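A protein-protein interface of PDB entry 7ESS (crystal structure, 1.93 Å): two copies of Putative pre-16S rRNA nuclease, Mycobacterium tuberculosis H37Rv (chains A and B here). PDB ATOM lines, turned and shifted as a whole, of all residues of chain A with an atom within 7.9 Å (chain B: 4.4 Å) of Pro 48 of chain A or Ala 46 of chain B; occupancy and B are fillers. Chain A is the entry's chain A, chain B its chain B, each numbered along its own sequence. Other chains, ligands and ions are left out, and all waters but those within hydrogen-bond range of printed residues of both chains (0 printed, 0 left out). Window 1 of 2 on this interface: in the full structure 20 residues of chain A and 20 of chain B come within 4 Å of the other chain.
The side-chain amide nitrogen (NE2) of Gln 151 of chain B sits at hydrogen-bond distance from the backbone carbonyl oxygen (O) of Ile 44 of chain B.
N of Ala 46 of chain B sits at hydrogen-bond distance from OE1 of Gln 151 of chain B (3.0 Å).
The backbone carbonyl oxygen of Thr 47 of chain B is in hydrogen-bond range of the backbone NH of Cys 38 of chain B, 2.8 Å away.
The side-chain hydroxyl (OG1) of Thr 51 of chain A is in hydrogen-bond range of the side-chain amide nitrogen (NE2) of Gln 143 of chain A (3.1 Å).
The backbone NH (N) of Cys 38 of chain A lies within hydrogen-bond range of the backbone carbonyl oxygen (O) of Thr 47 of chain A, 2.8 Å away.
Of the 10 printed residues of chain B, 6 touch a printed residue of chain A.
Printed residues of chain B that touch a printed residue of chain A: Ile 44, Leu 45, Ala 46, Thr 47, Pro 48 and Gln 151.
Hydrophobic or aromatic side chains of chain B that line the printed part of chain A: Ile 44, Leu 45 and Pro 48.
Of the 22 printed residues of chain A, 8 touch a printed residue of chain B.
Pro 48 of chain A touches three residues of chain B.
Ala 46 of chain B touches just one residue of chain A: Pro 48.
Leu 45 of chain B touches four residues of chain A.
Printed residues of chain B within 4 Å of Gln 143 of chain A: Leu 45 (3.4 Å).
Of the printed residues of chain B, Ile 141 of chain A touches Ile 44 (3.4 Å) and Gln 151 (3.98 Å).
Of the printed residues of chain A, Thr 47 of chain B touches Thr 47 and Pro 48.
The nearest residue of chain A that does not touch Ala 46 of chain B is Val 147 of chain A (5.2 Å).
The nearest printed residue of chain A that does not touch Thr 47 of chain B is Gln 143 of chain A (6.3 Å).
Leu 45 of chain A touches Pro 48 of chain B, and with the chains exchanged Pro 48 of chain A touches Leu 45 of chain B.
Ala 46 of chain A touches Pro 48 of chain B, and with the chains exchanged Pro 48 of chain A touches Ala 46 of chain B.
Thr 47 of chain A touches its own counterpart, Thr 47 of chain B.
Thr 47 of chain A touches Pro 48 of chain B, and with the chains exchanged Pro 48 of chain A touches Thr 47 of chain B.
Among the printed residues, pairs that only touch across the chains: Thr 47 of chain A with Pro 48 of chain B (3.3 Å), Pro 48 of chain A with Thr 47 of chain B (3.3 Å), Ile 141 of chain A with Ile 44 of chain B (3.4 Å), Gln 143 of chain A with Leu 45 of chain B (3.4 Å), Val 140 of chain A with Leu 45 of chain B (3.4 Å), Thr 47 of chain A with Thr 47 of chain B (3.5 Å), Ala 144 of chain A with Leu 45 of chain B (3.6 Å), Ala 144 of chain A with Gln 151 of chain B (3.6 Å), Leu 45 of chain A with Pro 48 of chain B (3.8 Å), Pro 48 of chain A with Leu 45 of chain B (3.8 Å), Pro 48 of chain A with Ala 46 of chain B (3.8 Å), Ala 46 of chain A with Pro 48 of chain B (3.9 Å) and Ile 141 of chain A with Gln 151 of chain B (3.98 Å).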
ATOM      1  N   GLY A  26       9.117  -6.662 -14.845  1.00  0.00           N
ATOM      2  CA  GLY A  26       9.633  -5.820 -13.807  1.00  0.00           C
ATOM      3  C   GLY A  26       9.468  -6.483 -12.462  1.00  0.00           C
ATOM      4  O   GLY A  26       8.424  -7.095 -12.229  1.00  0.00           O
ATOM      5  N   GLY A  35       7.433  -9.112  -6.123  1.00  0.00           N
ATOM      6  CA  GLY A  35       6.337  -8.676  -6.954  1.00  0.00           C
ATOM      7  C   GLY A  35       6.783  -8.636  -8.393  1.00  0.00           C
ATOM      8  O   GLY A  35       7.894  -8.253  -8.658  1.00  0.00           O
ATOM      9  N   VAL A  36       5.900  -9.000  -9.295  1.00  0.00           N
ATOM     10  CA  VAL A  36       6.214  -9.026 -10.680  1.00  0.00           C
ATOM     11  C   VAL A  36       5.150  -8.284 -11.476  1.00  0.00           C
ATOM     12  O   VAL A  36       3.932  -8.471 -11.290  1.00  0.00           O
ATOM     13  CB  VAL A  36       6.356 -10.456 -11.203  1.00  0.00           C
ATOM     14  CG1 VAL A  36       6.770 -10.480 -12.678  1.00  0.00           C
ATOM     15  CG2 VAL A  36       7.353 -11.234 -10.374  1.00  0.00           C
ATOM     16  N   ALA A  37       5.652  -7.516 -12.447  1.00  0.00           N
ATOM     17  CA  ALA A  37       4.850  -6.809 -13.403  1.00  0.00           C
ATOM     18  C   ALA A  37       5.384  -7.101 -14.814  1.00  0.00           C
ATOM     19  O   ALA A  37       6.505  -7.645 -14.943  1.00  0.00           O
ATOM     20  CB  ALA A  37       4.859  -5.327 -13.068  1.00  0.00           C
ATOM     21  N   CYS A  38       4.577  -6.812 -15.827  1.00  0.00           N
ATOM     22  CA  CYS A  38       5.078  -6.907 -17.203  1.00  0.00           C
ATOM     23  C   CYS A  38       4.505  -5.763 -18.038  1.00  0.00           C
ATOM     24  O   CYS A  38       3.559  -5.130 -17.649  1.00  0.00           O
ATOM     25  CB  CYS A  38       4.725  -8.243 -17.837  1.00  0.00           C
ATOM     26  SG  CYS A  38       2.976  -8.379 -18.276  1.00  0.00           S
ATOM     27  N   SER A  39       5.145  -5.484 -19.150  1.00  0.00           N
ATOM     28  CA  SER A  39       4.655  -4.478 -20.076  1.00  0.00           C
ATOM     29  C   SER A  39       3.907  -5.147 -21.239  1.00  0.00           C
ATOM     30  O   SER A  39       3.952  -6.348 -21.453  1.00  0.00           O
ATOM     31  CB  SER A  39       5.757  -3.574 -20.600  1.00  0.00           C
ATOM     32  OG  SER A  39       6.573  -4.213 -21.597  1.00  0.00           O
ATOM     33  N   LEU A  45       3.300   0.376 -21.104  1.00  0.00           N
ATOM     34  CA  LEU A  45       2.396   0.285 -19.942  1.00  0.00           C
ATOM     35  C   LEU A  45       2.719  -0.962 -19.120  1.00  0.00           C
ATOM     36  O   LEU A  45       2.690  -2.099 -19.662  1.00  0.00           O
ATOM     37  CB  LEU A  45       0.952   0.230 -20.475  1.00  0.00           C
ATOM     38  CG  LEU A  45      -0.173  -0.011 -19.464  1.00  0.00           C
ATOM     39  CD1 LEU A  45      -0.368   1.209 -18.572  1.00  0.00           C
ATOM     40  CD2 LEU A  45      -1.479  -0.366 -20.191  1.00  0.00           C
ATOM     41  N   ALA A  46       2.923  -0.770 -17.808  1.00  0.00           N
ATOM     42  CA  ALA A  46       3.138  -1.849 -16.861  1.00  0.00           C
ATOM     43  C   ALA A  46       1.803  -2.325 -16.271  1.00  0.00           C
ATOM     44  O   ALA A  46       0.972  -1.499 -15.884  1.00  0.00           O
ATOM     45  CB  ALA A  46       4.081  -1.364 -15.760  1.00  0.00           C
ATOM     46  N   THR A  47       1.659  -3.650 -16.157  1.00  0.00           N
ATOM     47  CA  THR A  47       0.522  -4.319 -15.589  1.00  0.00           C
ATOM     48  C   THR A  47       1.038  -5.342 -14.575  1.00  0.00           C
ATOM     49  O   THR A  47       2.067  -5.979 -14.828  1.00  0.00           O
ATOM     50  CB  THR A  47      -0.283  -5.042 -16.690  1.00  0.00           C
ATOM     51  OG1 THR A  47      -0.592  -4.148 -17.761  1.00  0.00           O
ATOM     52  CG2 THR A  47      -1.615  -5.558 -16.202  1.00  0.00           C
ATOM     53  N   PRO A  48       0.376  -5.483 -13.447  1.00  0.00           N
ATOM     54  CA  PRO A  48       0.808  -6.427 -12.426  1.00  0.00           C
ATOM     55  C   PRO A  48       0.579  -7.865 -12.886  1.00  0.00           C
ATOM     56  O   PRO A  48      -0.445  -8.110 -13.452  1.00  0.00           O
ATOM     57  CB  PRO A  48      -0.059  -6.108 -11.206  1.00  0.00           C
ATOM     58  CG  PRO A  48      -1.297  -5.435 -11.764  1.00  0.00           C
ATOM     59  CD  PRO A  48      -0.866  -4.790 -13.053  1.00  0.00           C
ATOM     60  N   VAL A  49       1.489  -8.799 -12.580  1.00  0.00           N
ATOM     61  CA  VAL A  49       1.343 -10.162 -13.034  1.00  0.00           C
ATOM     62  C   VAL A  49       1.147 -11.117 -11.860  1.00  0.00           C
ATOM     63  O   VAL A  49       0.195 -11.890 -11.835  1.00  0.00           O
ATOM     64  CB  VAL A  49       2.570 -10.572 -13.864  1.00  0.00           C
ATOM     65  CG1 VAL A  49       2.539 -12.054 -14.213  1.00  0.00           C
ATOM     66  CG2 VAL A  49       2.631  -9.724 -15.102  1.00  0.00           C
ATOM     67  N   GLU A  50       2.062 -11.124 -10.927  1.00  0.00           N
ATOM     68  CA  GLU A  50       2.036 -12.156  -9.931  1.00  0.00           C
ATOM     69  C   GLU A  50       2.978 -11.781  -8.781  1.00  0.00           C
ATOM     70  O   GLU A  50       3.840 -10.897  -8.870  1.00  0.00           O
ATOM     71  CB  GLU A  50       2.237 -13.522 -10.636  1.00  0.00           C
ATOM     72  CG  GLU A  50       3.432 -14.350 -10.279  1.00  0.00           C
ATOM     73  CD  GLU A  50       3.657 -15.631 -11.100  1.00  0.00           C
ATOM     74  OE1 GLU A  50       3.405 -15.631 -12.329  1.00  0.00           O
ATOM     75  OE2 GLU A  50       4.090 -16.628 -10.505  1.00  0.00           O
ATOM     76  N   THR A  51       2.772 -12.463  -7.683  1.00  0.00           N
ATOM     77  CA  THR A  51       3.664 -12.374  -6.579  1.00  0.00           C
ATOM     78  C   THR A  51       4.320 -13.746  -6.408  1.00  0.00           C
ATOM     79  O   THR A  51       3.633 -14.709  -6.159  1.00  0.00           O
ATOM     80  CB  THR A  51       2.964 -11.970  -5.279  1.00  0.00           C
ATOM     81  OG1 THR A  51       2.369 -10.691  -5.475  1.00  0.00           O
ATOM     82  CG2 THR A  51       3.932 -11.865  -4.128  1.00  0.00           C
ATOM     83  N   VAL A 140      -0.551  -9.826  -2.721  1.00  0.00           N
ATOM     84  CA  VAL A 140      -0.874  -9.223  -3.999  1.00  0.00           C
ATOM     85  C   VAL A 140      -0.323  -7.782  -4.074  1.00  0.00           C
ATOM     86  O   VAL A 140       0.040  -7.303  -5.158  1.00  0.00           O
ATOM     87  CB  VAL A 140      -2.390  -9.297  -4.225  1.00  0.00           C
ATOM     88  CG1 VAL A 140      -2.825  -8.519  -5.445  1.00  0.00           C
ATOM     89  CG2 VAL A 140      -2.855 -10.749  -4.317  1.00  0.00           C
ATOM     90  N   ILE A 141      -0.209  -7.084  -2.948  1.00  0.00           N
ATOM     91  CA  ILE A 141       0.088  -5.629  -3.046  1.00  0.00           C
ATOM     92  C   ILE A 141       1.549  -5.417  -3.447  1.00  0.00           C
ATOM     93  O   ILE A 141       1.908  -4.342  -3.913  1.00  0.00           O
ATOM     94  CB  ILE A 141      -0.276  -4.804  -1.791  1.00  0.00           C
ATOM     95  CG1 ILE A 141      -0.354  -3.319  -2.179  1.00  0.00           C
ATOM     96  CG2 ILE A 141       0.716  -5.034  -0.660  1.00  0.00           C
ATOM     97  CD1 ILE A 141      -1.398  -2.487  -1.463  1.00  0.00           C
ATOM     98  N   ASP A 142       2.377  -6.444  -3.337  1.00  0.00           N
ATOM     99  CA  ASP A 142       3.754  -6.365  -3.786  1.00  0.00           C
ATOM    100  C   ASP A 142       3.817  -6.138  -5.298  1.00  0.00           C
ATOM    101  O   ASP A 142       4.789  -5.570  -5.830  1.00  0.00           O
ATOM    102  CB  ASP A 142       4.527  -7.628  -3.395  1.00  0.00           C
ATOM    103  CG  ASP A 142       4.911  -7.690  -1.922  1.00  0.00           C
ATOM    104  OD1 ASP A 142       5.111  -6.633  -1.317  1.00  0.00           O
ATOM    105  OD2 ASP A 142       5.030  -8.796  -1.402  1.00  0.00           O
ATOM    106  N   GLN A 143       2.779  -6.507  -6.003  1.00  0.00           N
ATOM    107  CA  GLN A 143       2.785  -6.232  -7.443  1.00  0.00           C
ATOM    108  C   GLN A 143       2.657  -4.727  -7.698  1.00  0.00           C
ATOM    109  O   GLN A 143       2.959  -4.301  -8.777  1.00  0.00           O
ATOM    110  CB  GLN A 143       1.654  -6.985  -8.133  1.00  0.00           C
ATOM    111  CG  GLN A 143       1.803  -8.496  -7.961  1.00  0.00           C
ATOM    112  CD  GLN A 143       0.559  -9.225  -8.397  1.00  0.00           C
ATOM    113  OE1 GLN A 143      -0.148  -8.791  -9.307  1.00  0.00           O
ATOM    114  NE2 GLN A 143       0.285 -10.341  -7.737  1.00  0.00           N
ATOM    115  N   ALA A 144       2.105  -3.955  -6.769  1.00  0.00           N
ATOM    116  CA  ALA A 144       1.957  -2.507  -7.034  1.00  0.00           C
ATOM    117  C   ALA A 144       3.335  -1.829  -7.131  1.00  0.00           C
ATOM    118  O   ALA A 144       3.520  -0.896  -7.964  1.00  0.00           O
ATOM    119  CB  ALA A 144       1.097  -1.855  -5.990  1.00  0.00           C
ATOM    120  N   ALA A 145       4.315  -2.295  -6.339  1.00  0.00           N
ATOM    121  CA  ALA A 145       5.705  -1.790  -6.390  1.00  0.00           C
ATOM    122  C   ALA A 145       6.379  -2.162  -7.708  1.00  0.00           C
ATOM    123  O   ALA A 145       7.088  -1.343  -8.313  1.00  0.00           O
ATOM    124  CB  ALA A 145       6.519  -2.316  -5.230  1.00  0.00           C
ATOM    125  N   ALA A 146       6.159  -3.397  -8.127  1.00  0.00           N
ATOM    126  CA  ALA A 146       6.686  -3.858  -9.392  1.00  0.00           C
ATOM    127  C   ALA A 146       6.155  -3.001 -10.557  1.00  0.00           C
ATOM    128  O   ALA A 146       6.902  -2.667 -11.489  1.00  0.00           O
ATOM    129  CB  ALA A 146       6.370  -5.317  -9.557  1.00  0.00           C
ATOM    130  N   VAL A 147       4.878  -2.670 -10.526  1.00  0.00           N
ATOM    131  CA  VAL A 147       4.292  -1.870 -11.566  1.00  0.00           C
ATOM    132  C   VAL A 147       4.961  -0.486 -11.597  1.00  0.00           C
ATOM    133  O   VAL A 147       5.291   0.023 -12.669  1.00  0.00           O
ATOM    134  CB  VAL A 147       2.760  -1.786 -11.404  1.00  0.00           C
ATOM    135  CG1 VAL A 147       2.159  -0.696 -12.269  1.00  0.00           C
ATOM    136  CG2 VAL A 147       2.068  -3.110 -11.670  1.00  0.00           C
ATOM    137  N   LEU A 150       8.588  -0.682 -12.785  1.00  0.00           N
ATOM    138  CA  LEU A 150       8.631  -0.972 -14.235  1.00  0.00           C
ATOM    139  C   LEU A 150       8.135   0.241 -15.050  1.00  0.00           C
ATOM    140  O   LEU A 150       8.738   0.586 -16.074  1.00  0.00           O
ATOM    141  CB  LEU A 150       7.795  -2.209 -14.566  1.00  0.00           C
ATOM    142  CG  LEU A 150       7.715  -2.529 -16.065  1.00  0.00           C
ATOM    143  CD1 LEU A 150       9.135  -2.718 -16.605  1.00  0.00           C
ATOM    144  CD2 LEU A 150       6.899  -3.794 -16.296  1.00  0.00           C
ATOM    145  N   CYS B  38      -8.735  -0.589 -12.808  1.00  0.00           N
ATOM    146  CA  CYS B  38      -9.661  -1.149 -11.828  1.00  0.00           C
ATOM    147  C   CYS B  38      -8.899  -1.933 -10.758  1.00  0.00           C
ATOM    148  O   CYS B  38      -7.795  -2.370 -10.990  1.00  0.00           O
ATOM    149  CB  CYS B  38     -10.688  -2.062 -12.483  1.00  0.00           C
ATOM    150  SG  CYS B  38     -10.008  -3.658 -13.011  1.00  0.00           S
ATOM    151  N   ILE B  44      -7.146  -3.720  -3.243  1.00  0.00           N
ATOM    152  CA  ILE B  44      -5.737  -3.756  -2.865  1.00  0.00           C
ATOM    153  C   ILE B  44      -4.870  -3.187  -3.996  1.00  0.00           C
ATOM    154  O   ILE B  44      -3.925  -2.396  -3.744  1.00  0.00           O
ATOM    155  CB  ILE B  44      -5.340  -5.223  -2.546  1.00  0.00           C
ATOM    156  CG1 ILE B  44      -6.160  -5.784  -1.386  1.00  0.00           C
ATOM    157  CG2 ILE B  44      -3.862  -5.368  -2.282  1.00  0.00           C
ATOM    158  CD1 ILE B  44      -6.230  -4.860  -0.201  1.00  0.00           C
ATOM    159  N   LEU B  45      -5.138  -3.665  -5.222  1.00  0.00           N
ATOM    160  CA  LEU B  45      -4.187  -3.561  -6.345  1.00  0.00           C
ATOM    161  C   LEU B  45      -4.907  -3.060  -7.598  1.00  0.00           C
ATOM    162  O   LEU B  45      -5.900  -3.683  -8.070  1.00  0.00           O
ATOM    163  CB  LEU B  45      -3.558  -4.933  -6.607  1.00  0.00           C
ATOM    164  CG  LEU B  45      -2.679  -5.029  -7.857  1.00  0.00           C
ATOM    165  CD1 LEU B  45      -1.383  -4.268  -7.650  1.00  0.00           C
ATOM    166  CD2 LEU B  45      -2.387  -6.478  -8.189  1.00  0.00           C
ATOM    167  N   ALA B  46      -4.364  -1.953  -8.145  1.00  0.00           N
ATOM    168  CA  ALA B  46      -4.827  -1.353  -9.378  1.00  0.00           C
ATOM    169  C   ALA B  46      -4.145  -1.988 -10.596  1.00  0.00           C
ATOM    170  O   ALA B  46      -2.931  -2.154 -10.637  1.00  0.00           O
ATOM    171  CB  ALA B  46      -4.617   0.140  -9.376  1.00  0.00           C
ATOM    172  N   THR B  47      -4.984  -2.363 -11.563  1.00  0.00           N
ATOM    173  CA  THR B  47      -4.563  -2.932 -12.883  1.00  0.00           C
ATOM    174  C   THR B  47      -5.165  -2.079 -14.008  1.00  0.00           C
ATOM    175  O   THR B  47      -6.297  -1.603 -13.868  1.00  0.00           O
ATOM    176  CB  THR B  47      -5.027  -4.397 -13.004  1.00  0.00           C
ATOM    177  OG1 THR B  47      -4.555  -5.114 -11.862  1.00  0.00           O
ATOM    178  CG2 THR B  47      -4.518  -5.090 -14.245  1.00  0.00           C
ATOM    179  N   PRO B  48      -4.449  -1.870 -15.115  1.00  0.00           N
ATOM    180  CA  PRO B  48      -4.983  -1.130 -16.263  1.00  0.00           C
ATOM    181  C   PRO B  48      -6.143  -1.891 -16.921  1.00  0.00           C
ATOM    182  O   PRO B  48      -6.147  -3.072 -16.865  1.00  0.00           O
ATOM    183  CB  PRO B  48      -3.819  -0.955 -17.263  1.00  0.00           C
ATOM    184  CG  PRO B  48      -2.758  -1.903 -16.819  1.00  0.00           C
ATOM    185  CD  PRO B  48      -3.042  -2.239 -15.379  1.00  0.00           C
ATOM    186  N   VAL B 147      -3.856   3.884 -13.323  1.00  0.00           N
ATOM    187  CA  VAL B 147      -3.361   2.941 -12.338  1.00  0.00           C
ATOM    188  C   VAL B 147      -2.761   3.698 -11.133  1.00  0.00           C
ATOM    189  O   VAL B 147      -3.043   3.326 -10.024  1.00  0.00           O
ATOM    190  CB  VAL B 147      -2.341   1.975 -12.971  1.00  0.00           C
ATOM    191  CG1 VAL B 147      -1.599   1.194 -11.908  1.00  0.00           C
ATOM    192  CG2 VAL B 147      -2.978   1.029 -13.988  1.00  0.00           C
ATOM    193  N   LEU B 150      -5.480   5.469  -9.012  1.00  0.00           N
ATOM    194  CA  LEU B 150      -6.284   4.495  -8.328  1.00  0.00           C
ATOM    195  C   LEU B 150      -5.471   3.826  -7.218  1.00  0.00           C
ATOM    196  O   LEU B 150      -5.985   3.702  -6.081  1.00  0.00           O
ATOM    197  CB  LEU B 150      -6.852   3.475  -9.321  1.00  0.00           C
ATOM    198  CG  LEU B 150      -7.658   2.357  -8.649  1.00  0.00           C
ATOM    199  CD1 LEU B 150      -8.761   2.979  -7.785  1.00  0.00           C
ATOM    200  CD2 LEU B 150      -8.239   1.372  -9.675  1.00  0.00           C
ATOM    201  N   GLN B 151      -4.200   3.448  -7.496  1.00  0.00           N
ATOM    202  CA  GLN B 151      -3.414   2.813  -6.465  1.00  0.00           C
ATOM    203  C   GLN B 151      -3.254   3.783  -5.285  1.00  0.00           C
ATOM    204  O   GLN B 151      -3.239   3.349  -4.165  1.00  0.00           O
ATOM    205  CB  GLN B 151      -2.032   2.402  -6.967  1.00  0.00           C
ATOM    206  CG  GLN B 151      -1.257   1.529  -5.982  1.00  0.00           C
ATOM    207  CD  GLN B 151      -1.950   0.211  -5.782  1.00  0.00           C
ATOM    208  OE1 GLN B 151      -2.182  -0.505  -6.750  1.00  0.00           O
ATOM    209  NE2 GLN B 151      -2.283  -0.110  -4.533  1.00  0.00           N
ATOM    210  N   LEU B 154      -6.332   3.582  -3.188  1.00  0.00           N
ATOM    211  CA  LEU B 154      -6.382   2.295  -2.468  1.00  0.00           C
ATOM    212  C   LEU B 154      -5.418   2.278  -1.261  1.00  0.00           C
ATOM    213  O   LEU B 154      -5.812   1.807  -0.147  1.00  0.00           O
ATOM    214  CB  LEU B 154      -6.046   1.149  -3.430  1.00  0.00           C
ATOM    215  CG  LEU B 154      -6.963   1.006  -4.648  1.00  0.00           C
ATOM    216  CD1 LEU B 154      -6.505  -0.155  -5.522  1.00  0.00           C
ATOM    217  CD2 LEU B 154      -8.415   0.838  -4.249  1.00  0.00           C
